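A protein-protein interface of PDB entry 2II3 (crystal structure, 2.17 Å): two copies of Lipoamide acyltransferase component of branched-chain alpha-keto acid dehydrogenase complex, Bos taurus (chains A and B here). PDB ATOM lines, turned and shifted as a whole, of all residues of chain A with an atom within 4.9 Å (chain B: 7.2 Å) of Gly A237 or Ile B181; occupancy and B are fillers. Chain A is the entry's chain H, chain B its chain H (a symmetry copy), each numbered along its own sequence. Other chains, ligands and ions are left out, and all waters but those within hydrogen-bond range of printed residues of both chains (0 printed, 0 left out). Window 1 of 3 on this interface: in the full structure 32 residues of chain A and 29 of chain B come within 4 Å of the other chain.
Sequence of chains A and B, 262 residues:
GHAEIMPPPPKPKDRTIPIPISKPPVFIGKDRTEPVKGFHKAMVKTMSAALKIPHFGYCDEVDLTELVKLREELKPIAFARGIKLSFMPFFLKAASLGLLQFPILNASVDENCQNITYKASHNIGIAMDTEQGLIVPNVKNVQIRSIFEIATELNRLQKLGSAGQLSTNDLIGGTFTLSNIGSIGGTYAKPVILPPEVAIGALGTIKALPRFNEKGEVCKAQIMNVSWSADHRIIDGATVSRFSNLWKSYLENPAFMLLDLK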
ATOM      1  N   PHE A  56     -31.220  19.071 -13.064  1.00  0.00           N
ATOM      2  CA  PHE A  56     -30.056  18.189 -13.210  1.00  0.00           C
ATOM      3  C   PHE A  56     -30.675  16.892 -13.724  1.00  0.00           C
ATOM      4  O   PHE A  56     -31.704  16.506 -13.225  1.00  0.00           O
ATOM      5  CB  PHE A  56     -29.442  17.993 -11.804  1.00  0.00           C
ATOM      6  CG  PHE A  56     -28.490  16.826 -11.690  1.00  0.00           C
ATOM      7  CD1 PHE A  56     -27.272  16.840 -12.362  1.00  0.00           C
ATOM      8  CD2 PHE A  56     -28.828  15.715 -10.893  1.00  0.00           C
ATOM      9  CE1 PHE A  56     -26.387  15.745 -12.258  1.00  0.00           C
ATOM     10  CE2 PHE A  56     -27.990  14.631 -10.801  1.00  0.00           C
ATOM     11  CZ  PHE A  56     -26.733  14.656 -11.471  1.00  0.00           C
ATOM     12  N   TYR A  58     -30.291  12.627 -14.206  1.00  0.00           N
ATOM     13  CA  TYR A  58     -29.510  11.475 -13.788  1.00  0.00           C
ATOM     14  C   TYR A  58     -30.309  10.253 -14.266  1.00  0.00           C
ATOM     15  O   TYR A  58     -31.479  10.123 -13.943  1.00  0.00           O
ATOM     16  CB  TYR A  58     -29.378  11.472 -12.252  1.00  0.00           C
ATOM     17  CG  TYR A  58     -28.829  10.159 -11.673  1.00  0.00           C
ATOM     18  CD1 TYR A  58     -29.683   9.097 -11.364  1.00  0.00           C
ATOM     19  CD2 TYR A  58     -27.446   9.946 -11.579  1.00  0.00           C
ATOM     20  CE1 TYR A  58     -29.184   7.859 -10.946  1.00  0.00           C
ATOM     21  CE2 TYR A  58     -26.951   8.722 -11.142  1.00  0.00           C
ATOM     22  CZ  TYR A  58     -27.808   7.703 -10.812  1.00  0.00           C
ATOM     23  OH  TYR A  58     -27.264   6.518 -10.340  1.00  0.00           O
ATOM     24  N   HIS A 232     -31.550  21.170  -8.904  1.00  0.00           N
ATOM     25  CA  HIS A 232     -30.205  21.151  -8.325  1.00  0.00           C
ATOM     26  C   HIS A 232     -29.888  22.347  -7.399  1.00  0.00           C
ATOM     27  O   HIS A 232     -28.780  22.447  -6.879  1.00  0.00           O
ATOM     28  CB  HIS A 232     -29.131  20.977  -9.408  1.00  0.00           C
ATOM     29  CG  HIS A 232     -27.935  20.174  -8.941  1.00  0.00           C
ATOM     30  ND1 HIS A 232     -27.333  20.371  -7.712  1.00  0.00           N
ATOM     31  CD2 HIS A 232     -27.226  19.189  -9.542  1.00  0.00           C
ATOM     32  CE1 HIS A 232     -26.312  19.537  -7.575  1.00  0.00           C
ATOM     33  NE2 HIS A 232     -26.230  18.809  -8.669  1.00  0.00           N
ATOM     34  N   ILE A 235     -31.297  19.798  -4.491  1.00  0.00           N
ATOM     35  CA  ILE A 235     -31.039  18.353  -4.596  1.00  0.00           C
ATOM     36  C   ILE A 235     -29.676  18.107  -5.268  1.00  0.00           C
ATOM     37  O   ILE A 235     -29.442  18.580  -6.370  1.00  0.00           O
ATOM     38  CB  ILE A 235     -32.103  17.561  -5.412  1.00  0.00           C
ATOM     39  CG1 ILE A 235     -33.575  17.852  -5.004  1.00  0.00           C
ATOM     40  CG2 ILE A 235     -31.783  16.076  -5.352  1.00  0.00           C
ATOM     41  CD1 ILE A 235     -33.885  17.634  -3.607  1.00  0.00           C
ATOM     42  N   ASP A 236     -28.778  17.387  -4.601  1.00  0.00           N
ATOM     43  CA  ASP A 236     -27.460  17.160  -5.179  1.00  0.00           C
ATOM     44  C   ASP A 236     -27.420  15.844  -5.913  1.00  0.00           C
ATOM     45  O   ASP A 236     -28.330  15.015  -5.775  1.00  0.00           O
ATOM     46  CB  ASP A 236     -26.309  17.369  -4.150  1.00  0.00           C
ATOM     47  CG  ASP A 236     -26.341  16.387  -2.976  1.00  0.00           C
ATOM     48  OD1 ASP A 236     -26.780  15.236  -3.166  1.00  0.00           O
ATOM     49  OD2 ASP A 236     -25.902  16.762  -1.849  1.00  0.00           O
ATOM     50  N   GLY A 237     -26.396  15.667  -6.738  1.00  0.00           N
ATOM     51  CA  GLY A 237     -26.253  14.461  -7.550  1.00  0.00           C
ATOM     52  C   GLY A 237     -26.275  13.226  -6.691  1.00  0.00           C
ATOM     53  O   GLY A 237     -26.883  12.265  -7.056  1.00  0.00           O
ATOM     54  N   ALA A 238     -25.620  13.254  -5.541  1.00  0.00           N
ATOM     55  CA  ALA A 238     -25.538  12.083  -4.649  1.00  0.00           C
ATOM     56  C   ALA A 238     -26.876  11.615  -4.113  1.00  0.00           C
ATOM     57  O   ALA A 238     -27.112  10.430  -4.093  1.00  0.00           O
ATOM     58  CB  ALA A 238     -24.538  12.333  -3.478  1.00  0.00           C
ATOM     59  N   THR A 239     -27.719  12.541  -3.649  1.00  0.00           N
ATOM     60  CA  THR A 239     -29.075  12.229  -3.232  1.00  0.00           C
ATOM     61  C   THR A 239     -29.948  11.547  -4.315  1.00  0.00           C
ATOM     62  O   THR A 239     -30.640  10.540  -4.048  1.00  0.00           O
ATOM     63  CB  THR A 239     -29.769  13.512  -2.733  1.00  0.00           C
ATOM     64  OG1 THR A 239     -28.951  14.128  -1.729  1.00  0.00           O
ATOM     65  CG2 THR A 239     -31.149  13.214  -2.201  1.00  0.00           C
ATOM     66  N   VAL A 240     -29.907  12.067  -5.542  1.00  0.00           N
ATOM     67  CA  VAL A 240     -30.719  11.533  -6.606  1.00  0.00           C
ATOM     68  C   VAL A 240     -30.239  10.114  -6.941  1.00  0.00           C
ATOM     69  O   VAL A 240     -31.011   9.209  -7.194  1.00  0.00           O
ATOM     70  CB  VAL A 240     -30.585  12.422  -7.874  1.00  0.00           C
ATOM     71  CG1 VAL A 240     -31.379  11.800  -9.073  1.00  0.00           C
ATOM     72  CG2 VAL A 240     -31.165  13.794  -7.600  1.00  0.00           C
ATOM     73  N   SER A 241     -28.931   9.960  -6.977  1.00  0.00           N
ATOM     74  CA  SER A 241     -28.295   8.709  -7.277  1.00  0.00           C
ATOM     75  C   SER A 241     -28.542   7.604  -6.248  1.00  0.00           C
ATOM     76  O   SER A 241     -28.828   6.469  -6.586  1.00  0.00           O
ATOM     77  CB  SER A 241     -26.770   8.946  -7.302  1.00  0.00           C
ATOM     78  OG  SER A 241     -26.269   7.864  -8.042  1.00  0.00           O
ATOM     79  N   MET B  43     -25.109  26.491  -3.414  1.00  0.00           N
ATOM     80  CA  MET B  43     -25.578  25.637  -4.520  1.00  0.00           C
ATOM     81  C   MET B  43     -26.810  26.316  -5.160  1.00  0.00           C
ATOM     82  O   MET B  43     -26.957  26.336  -6.364  1.00  0.00           O
ATOM     83  CB  MET B  43     -25.888  24.217  -4.037  1.00  0.00           C
ATOM     84  CG  MET B  43     -26.093  23.254  -5.179  1.00  0.00           C
ATOM     85  SD  MET B  43     -26.251  21.539  -4.694  1.00  0.00           S
ATOM     86  CE  MET B  43     -27.754  21.568  -3.771  1.00  0.00           C
ATOM     87  N   MET B  88     -10.400   7.898 -12.291  1.00  0.00           N
ATOM     88  CA  MET B  88     -10.396   9.383 -12.451  1.00  0.00           C
ATOM     89  C   MET B  88      -9.074  10.028 -12.932  1.00  0.00           C
ATOM     90  O   MET B  88      -9.109  10.915 -13.749  1.00  0.00           O
ATOM     91  CB  MET B  88     -10.874  10.135 -11.165  1.00  0.00           C
ATOM     92  CG  MET B  88     -12.440  10.144 -10.916  1.00  0.00           C
ATOM     93  SD  MET B  88     -13.314  10.971 -12.304  1.00  0.00           S
ATOM     94  CE  MET B  88     -13.132  12.702 -11.878  1.00  0.00           C
ATOM     95  N   ALA B 127     -16.411  17.251  -9.054  1.00  0.00           N
ATOM     96  CA  ALA B 127     -17.644  17.542  -8.307  1.00  0.00           C
ATOM     97  C   ALA B 127     -17.749  16.466  -7.224  1.00  0.00           C
ATOM     98  O   ALA B 127     -17.648  15.292  -7.536  1.00  0.00           O
ATOM     99  CB  ALA B 127     -18.846  17.528  -9.242  1.00  0.00           C
ATOM    100  N   ASP B 129     -19.955  15.602  -3.354  1.00  0.00           N
ATOM    101  CA  ASP B 129     -21.020  16.068  -2.439  1.00  0.00           C
ATOM    102  C   ASP B 129     -20.615  15.698  -1.002  1.00  0.00           C
ATOM    103  O   ASP B 129     -20.093  14.590  -0.733  1.00  0.00           O
ATOM    104  CB  ASP B 129     -22.417  15.487  -2.753  1.00  0.00           C
ATOM    105  CG  ASP B 129     -22.935  15.887  -4.121  1.00  0.00           C
ATOM    106  OD1 ASP B 129     -22.943  17.095  -4.420  1.00  0.00           O
ATOM    107  OD2 ASP B 129     -23.339  14.996  -4.911  1.00  0.00           O
ATOM    108  N   LEU B 134     -22.809  20.706  -2.561  1.00  0.00           N
ATOM    109  CA  LEU B 134     -21.900  20.528  -3.666  1.00  0.00           C
ATOM    110  C   LEU B 134     -20.589  21.268  -3.365  1.00  0.00           C
ATOM    111  O   LEU B 134     -20.594  22.456  -3.087  1.00  0.00           O
ATOM    112  CB  LEU B 134     -22.528  21.095  -4.955  1.00  0.00           C
ATOM    113  CG  LEU B 134     -21.678  21.124  -6.236  1.00  0.00           C
ATOM    114  CD1 LEU B 134     -21.242  19.727  -6.677  1.00  0.00           C
ATOM    115  CD2 LEU B 134     -22.407  21.860  -7.367  1.00  0.00           C
ATOM    116  N   LEU B 178     -15.287  17.585 -14.228  1.00  0.00           N
ATOM    117  CA  LEU B 178     -15.784  16.220 -14.379  1.00  0.00           C
ATOM    118  C   LEU B 178     -16.527  15.828 -13.134  1.00  0.00           C
ATOM    119  O   LEU B 178     -16.125  16.208 -12.013  1.00  0.00           O
ATOM    120  CB  LEU B 178     -14.660  15.203 -14.636  1.00  0.00           C
ATOM    121  CG  LEU B 178     -13.853  15.387 -15.903  1.00  0.00           C
ATOM    122  CD1 LEU B 178     -12.689  14.431 -15.904  1.00  0.00           C
ATOM    123  CD2 LEU B 178     -14.737  15.169 -17.079  1.00  0.00           C
ATOM    124  N   SER B 179     -17.608  15.088 -13.322  1.00  0.00           N
ATOM    125  CA  SER B 179     -18.423  14.611 -12.195  1.00  0.00           C
ATOM    126  C   SER B 179     -18.532  13.068 -12.288  1.00  0.00           C
ATOM    127  O   SER B 179     -19.147  12.539 -13.208  1.00  0.00           O
ATOM    128  CB  SER B 179     -19.792  15.319 -12.220  1.00  0.00           C
ATOM    129  OG  SER B 179     -20.646  14.884 -11.144  1.00  0.00           O
ATOM    130  N   ASN B 180     -17.894  12.345 -11.393  1.00  0.00           N
ATOM    131  CA  ASN B 180     -17.968  10.883 -11.397  1.00  0.00           C
ATOM    132  C   ASN B 180     -19.252  10.407 -10.733  1.00  0.00           C
ATOM    133  O   ASN B 180     -19.236   9.884  -9.647  1.00  0.00           O
ATOM    134  CB  ASN B 180     -16.743  10.253 -10.696  1.00  0.00           C
ATOM    135  CG  ASN B 180     -16.607   8.761 -11.004  1.00  0.00           C
ATOM    136  OD1 ASN B 180     -17.310   8.213 -11.890  1.00  0.00           O
ATOM    137  ND2 ASN B 180     -15.741   8.079 -10.257  1.00  0.00           N
ATOM    138  N   ILE B 181     -20.393  10.571 -11.367  1.00  0.00           N
ATOM    139  CA  ILE B 181     -21.596  10.122 -10.681  1.00  0.00           C
ATOM    140  C   ILE B 181     -21.599   8.545 -10.574  1.00  0.00           C
ATOM    141  O   ILE B 181     -22.190   7.977  -9.656  1.00  0.00           O
ATOM    142  CB  ILE B 181     -22.888  10.772 -11.318  1.00  0.00           C
ATOM    143  CG1 ILE B 181     -24.133  10.616 -10.393  1.00  0.00           C
ATOM    144  CG2 ILE B 181     -23.104  10.216 -12.752  1.00  0.00           C
ATOM    145  CD1 ILE B 181     -23.895  10.707  -8.727  1.00  0.00           C
ATOM    146  N   GLY B 182     -20.877   7.884 -11.485  1.00  0.00           N
ATOM    147  CA  GLY B 182     -20.709   6.425 -11.482  1.00  0.00           C
ATOM    148  C   GLY B 182     -20.032   5.806 -10.273  1.00  0.00           C
ATOM    149  O   GLY B 182     -20.056   4.575 -10.109  1.00  0.00           O
ATOM    150  N   SER B 183     -19.443   6.630  -9.389  1.00  0.00           N
ATOM    151  CA  SER B 183     -18.845   6.060  -8.188  1.00  0.00           C
ATOM    152  C   SER B 183     -19.996   5.656  -7.285  1.00  0.00           C
ATOM    153  O   SER B 183     -19.794   4.866  -6.370  1.00  0.00           O
ATOM    154  CB  SER B 183     -17.932   7.043  -7.468  1.00  0.00           C
ATOM    155  OG  SER B 183     -18.587   8.261  -7.190  1.00  0.00           O
ATOM    156  N   ILE B 184     -21.203   6.192  -7.570  1.00  0.00           N
ATOM    157  CA  ILE B 184     -22.456   5.822  -6.909  1.00  0.00           C
ATOM    158  C   ILE B 184     -23.384   4.961  -7.827  1.00  0.00           C
ATOM    159  O   ILE B 184     -23.833   3.867  -7.451  1.00  0.00           O
ATOM    160  CB  ILE B 184     -23.225   7.065  -6.334  1.00  0.00           C
ATOM    161  CG1 ILE B 184     -22.265   8.006  -5.571  1.00  0.00           C
ATOM    162  CG2 ILE B 184     -24.420   6.597  -5.412  1.00  0.00           C
ATOM    163  CD1 ILE B 184     -22.915   9.172  -4.813  1.00  0.00           C
ATOM    164  N   GLY B 185     -23.711   5.452  -9.014  1.00  0.00           N
ATOM    165  CA  GLY B 185     -24.496   4.624  -9.936  1.00  0.00           C
ATOM    166  C   GLY B 185     -24.726   5.415 -11.204  1.00  0.00           C
ATOM    167  O   GLY B 185     -24.157   6.506 -11.356  1.00  0.00           O
ATOM    168  N   GLY B 186     -25.560   4.895 -12.116  1.00  0.00           N
ATOM    169  CA  GLY B 186     -26.056   5.736 -13.254  1.00  0.00           C
ATOM    170  C   GLY B 186     -25.456   5.322 -14.566  1.00  0.00           C
ATOM    171  O   GLY B 186     -24.458   4.585 -14.592  1.00  0.00           O
ATOM    172  N   THR B 187     -26.094   5.754 -15.656  1.00  0.00           N
ATOM    173  CA  THR B 187     -25.614   5.576 -16.985  1.00  0.00           C
ATOM    174  C   THR B 187     -25.351   6.946 -17.542  1.00  0.00           C
ATOM    175  O   THR B 187     -24.257   7.483 -17.358  1.00  0.00           O
ATOM    176  CB  THR B 187     -26.553   4.713 -17.853  1.00  0.00           C
ATOM    177  OG1 THR B 187     -27.854   5.287 -17.950  1.00  0.00           O
ATOM    178  CG2 THR B 187     -26.627   3.177 -17.383  1.00  0.00           C
ATOM    179  N   TYR B 188     -26.375   7.553 -18.160  1.00  0.00           N
ATOM    180  CA  TYR B 188     -26.318   8.882 -18.719  1.00  0.00           C
ATOM    181  C   TYR B 188     -26.763   9.888 -17.676  1.00  0.00           C
ATOM    182  O   TYR B 188     -27.347   9.519 -16.657  1.00  0.00           O
ATOM    183  CB  TYR B 188     -27.210   8.930 -19.992  1.00  0.00           C
ATOM    184  CG  TYR B 188     -26.620   8.141 -21.152  1.00  0.00           C
ATOM    185  CD1 TYR B 188     -25.434   8.571 -21.804  1.00  0.00           C
ATOM    186  CD2 TYR B 188     -27.205   6.968 -21.570  1.00  0.00           C
ATOM    187  CE1 TYR B 188     -24.914   7.852 -22.862  1.00  0.00           C
ATOM    188  CE2 TYR B 188     -26.662   6.218 -22.596  1.00  0.00           C
ATOM    189  CZ  TYR B 188     -25.547   6.661 -23.264  1.00  0.00           C
ATOM    190  OH  TYR B 188     -25.056   5.923 -24.331  1.00  0.00           O
ATOM    191  N   ALA B 189     -26.459  11.162 -17.918  1.00  0.00           N
ATOM    192  CA  ALA B 189     -26.872  12.259 -17.028  1.00  0.00           C
ATOM    193  C   ALA B 189     -27.038  13.525 -17.864  1.00  0.00           C
ATOM    194  O   ALA B 189     -26.636  13.537 -19.028  1.00  0.00           O
ATOM    195  CB  ALA B 189     -25.799  12.497 -15.938  1.00  0.00           C
ATOM    196  N   GLY B 201     -18.408  17.289 -17.861  1.00  0.00           N
ATOM    197  CA  GLY B 201     -18.835  15.931 -18.170  1.00  0.00           C
ATOM    198  C   GLY B 201     -19.184  15.069 -16.991  1.00  0.00           C
ATOM    199  O   GLY B 201     -18.577  15.223 -15.923  1.00  0.00           O
ATOM    200  N   ALA B 202     -20.088  14.087 -17.195  1.00  0.00           N
ATOM    201  CA  ALA B 202     -20.512  13.256 -16.134  1.00  0.00           C
ATOM    202  C   ALA B 202     -20.260  11.859 -16.599  1.00  0.00           C
ATOM    203  O   ALA B 202     -20.703  11.476 -17.688  1.00  0.00           O
ATOM    204  CB  ALA B 202     -21.973  13.461 -15.800  1.00  0.00           C
ATOM    205  N   LEU B 203     -19.577  11.094 -15.753  1.00  0.00           N
ATOM    206  CA  LEU B 203     -19.185   9.690 -16.055  1.00  0.00           C
ATOM    207  C   LEU B 203     -20.095   8.732 -15.341  1.00  0.00           C
ATOM    208  O   LEU B 203     -20.254   8.846 -14.145  1.00  0.00           O
ATOM    209  CB  LEU B 203     -17.735   9.443 -15.584  1.00  0.00           C
ATOM    210  CG  LEU B 203     -17.003  10.705 -16.081  1.00  0.00           C
ATOM    211  CD1 LEU B 203     -15.919  11.166 -15.171  1.00  0.00           C
ATOM    212  CD2 LEU B 203     -16.617  10.584 -17.593  1.00  0.00           C
ATOM    213  N   GLY B 204     -20.654   7.780 -16.064  1.00  0.00           N
ATOM    214  CA  GLY B 204     -21.480   6.778 -15.506  1.00  0.00           C
ATOM    215  C   GLY B 204     -20.752   5.595 -14.901  1.00  0.00           C
ATOM    216  O   GLY B 204     -19.499   5.576 -14.776  1.00  0.00           O
ATOM    217  N   THR B 205     -21.545   4.609 -14.498  1.00  0.00           N
ATOM    218  CA  THR B 205     -21.010   3.356 -13.915  1.00  0.00           C
ATOM    219  C   THR B 205     -20.343   2.493 -15.012  1.00  0.00           C
ATOM    220  O   THR B 205     -20.968   2.242 -16.085  1.00  0.00           O
ATOM    221  CB  THR B 205     -22.123   2.511 -13.254  1.00  0.00           C
ATOM    222  OG1 THR B 205     -22.807   3.311 -12.279  1.00  0.00           O
ATOM    223  CG2 THR B 205     -21.521   1.241 -12.508  1.00  0.00           C
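O of Gly B186 is in hydrogen-bond range of N of Thr B205 (2.9 Å). ND1 of His A232 lies within hydrogen-bond range of O of Ile A235, 3.1 Å away. The side-chain hydroxyl (OH) of Tyr A58 is in hydrogen-bond range of the side-chain hydroxyl (OG) of Ser A241, at 2.8 Å. The side-chain hydroxyl (OG1) of Thr A239 is in hydrogen-bond range of the side-chain carboxylate (OD1) of Asp A236 (2.8 Å). The backbone NH (N) of Ile B181 is in hydrogen-bond range of the backbone carbonyl oxygen (O) of Leu B203. The backbone NH (N) of Ala A238 sits close to the side-chain carboxylate (OD1) of Asp A236 (3.3 Å).
Printed residues of chain B that touch a printed residue of chain A: Met B43, Asp B129, Ile B181, Ile B184, Gly B185, Gly B186 and Tyr B188. Hydrophobic or aromatic side chains of chain A that line the printed part of chain B: Tyr A58, His A232 and Ala A238. Among the printed residues, 13 pairs touch across the chains.
No position is printed for both chains.
Of chain B, only Asp B129 and Ile B181 come within 4 Å of Gly A237. Ile B181 touches just these residues of chain A: Tyr A58, Gly A237 and Ser A241. Printed residues of chain B within 4 Å of Asp A236: Asp B129 (3.4 Å). Printed residues of chain B within 4 Å of Ala A238: Asp B129 (2.9 Å) and Ile B184 (3.8 Å). Of the printed residues of chain B, Tyr A58 touches Ile B181 (3.5 Å), Gly B185 (2.9 Å), Gly B186 (2.9 Å) and Tyr B188 (3.9 Å). Gly B204 touches none of the printed residues of chain A. The nearest printed residue of chain A that does not touch Asp B129 is Thr A239 (5.2 Å).
A ring nitrogen (ND1) of His A232 is in hydrogen-bond range of the side-chain sulfur of Met B43. OH of Tyr A58 sits close to O of Gly B185, 3.3 Å away. The side-chain hydroxyl of Tyr A58 sits at hydrogen-bond distance from the backbone NH of Gly B186 (2.9 Å). The side-chain carboxylate (OD2) of Asp B129 is in hydrogen-bond range of the backbone NH (N) of Ala A238, at 2.9 Å.
Tyr A58 touches Ile B181. C of Tyr A58 touches O of Tyr B188, at 3.9 Å. OD1 of Asp B129 touches CB of Asp A236, at 3.4 Å. Asp B129 touches Gly A237 (OD2 to N, 3.6 Å). CD1 of Ile B181 touches O of Gly A237 (3.8 Å). Ile B184 touches Ala A238 (CD1 to CB, 3.8 Å). Ser A241 touches Ile B181 (CB to CD1, 3.7 Å). CG2 of Ile B184 touches OG of Ser A241, at 3.5 Å. Ser A241 touches Gly B185.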
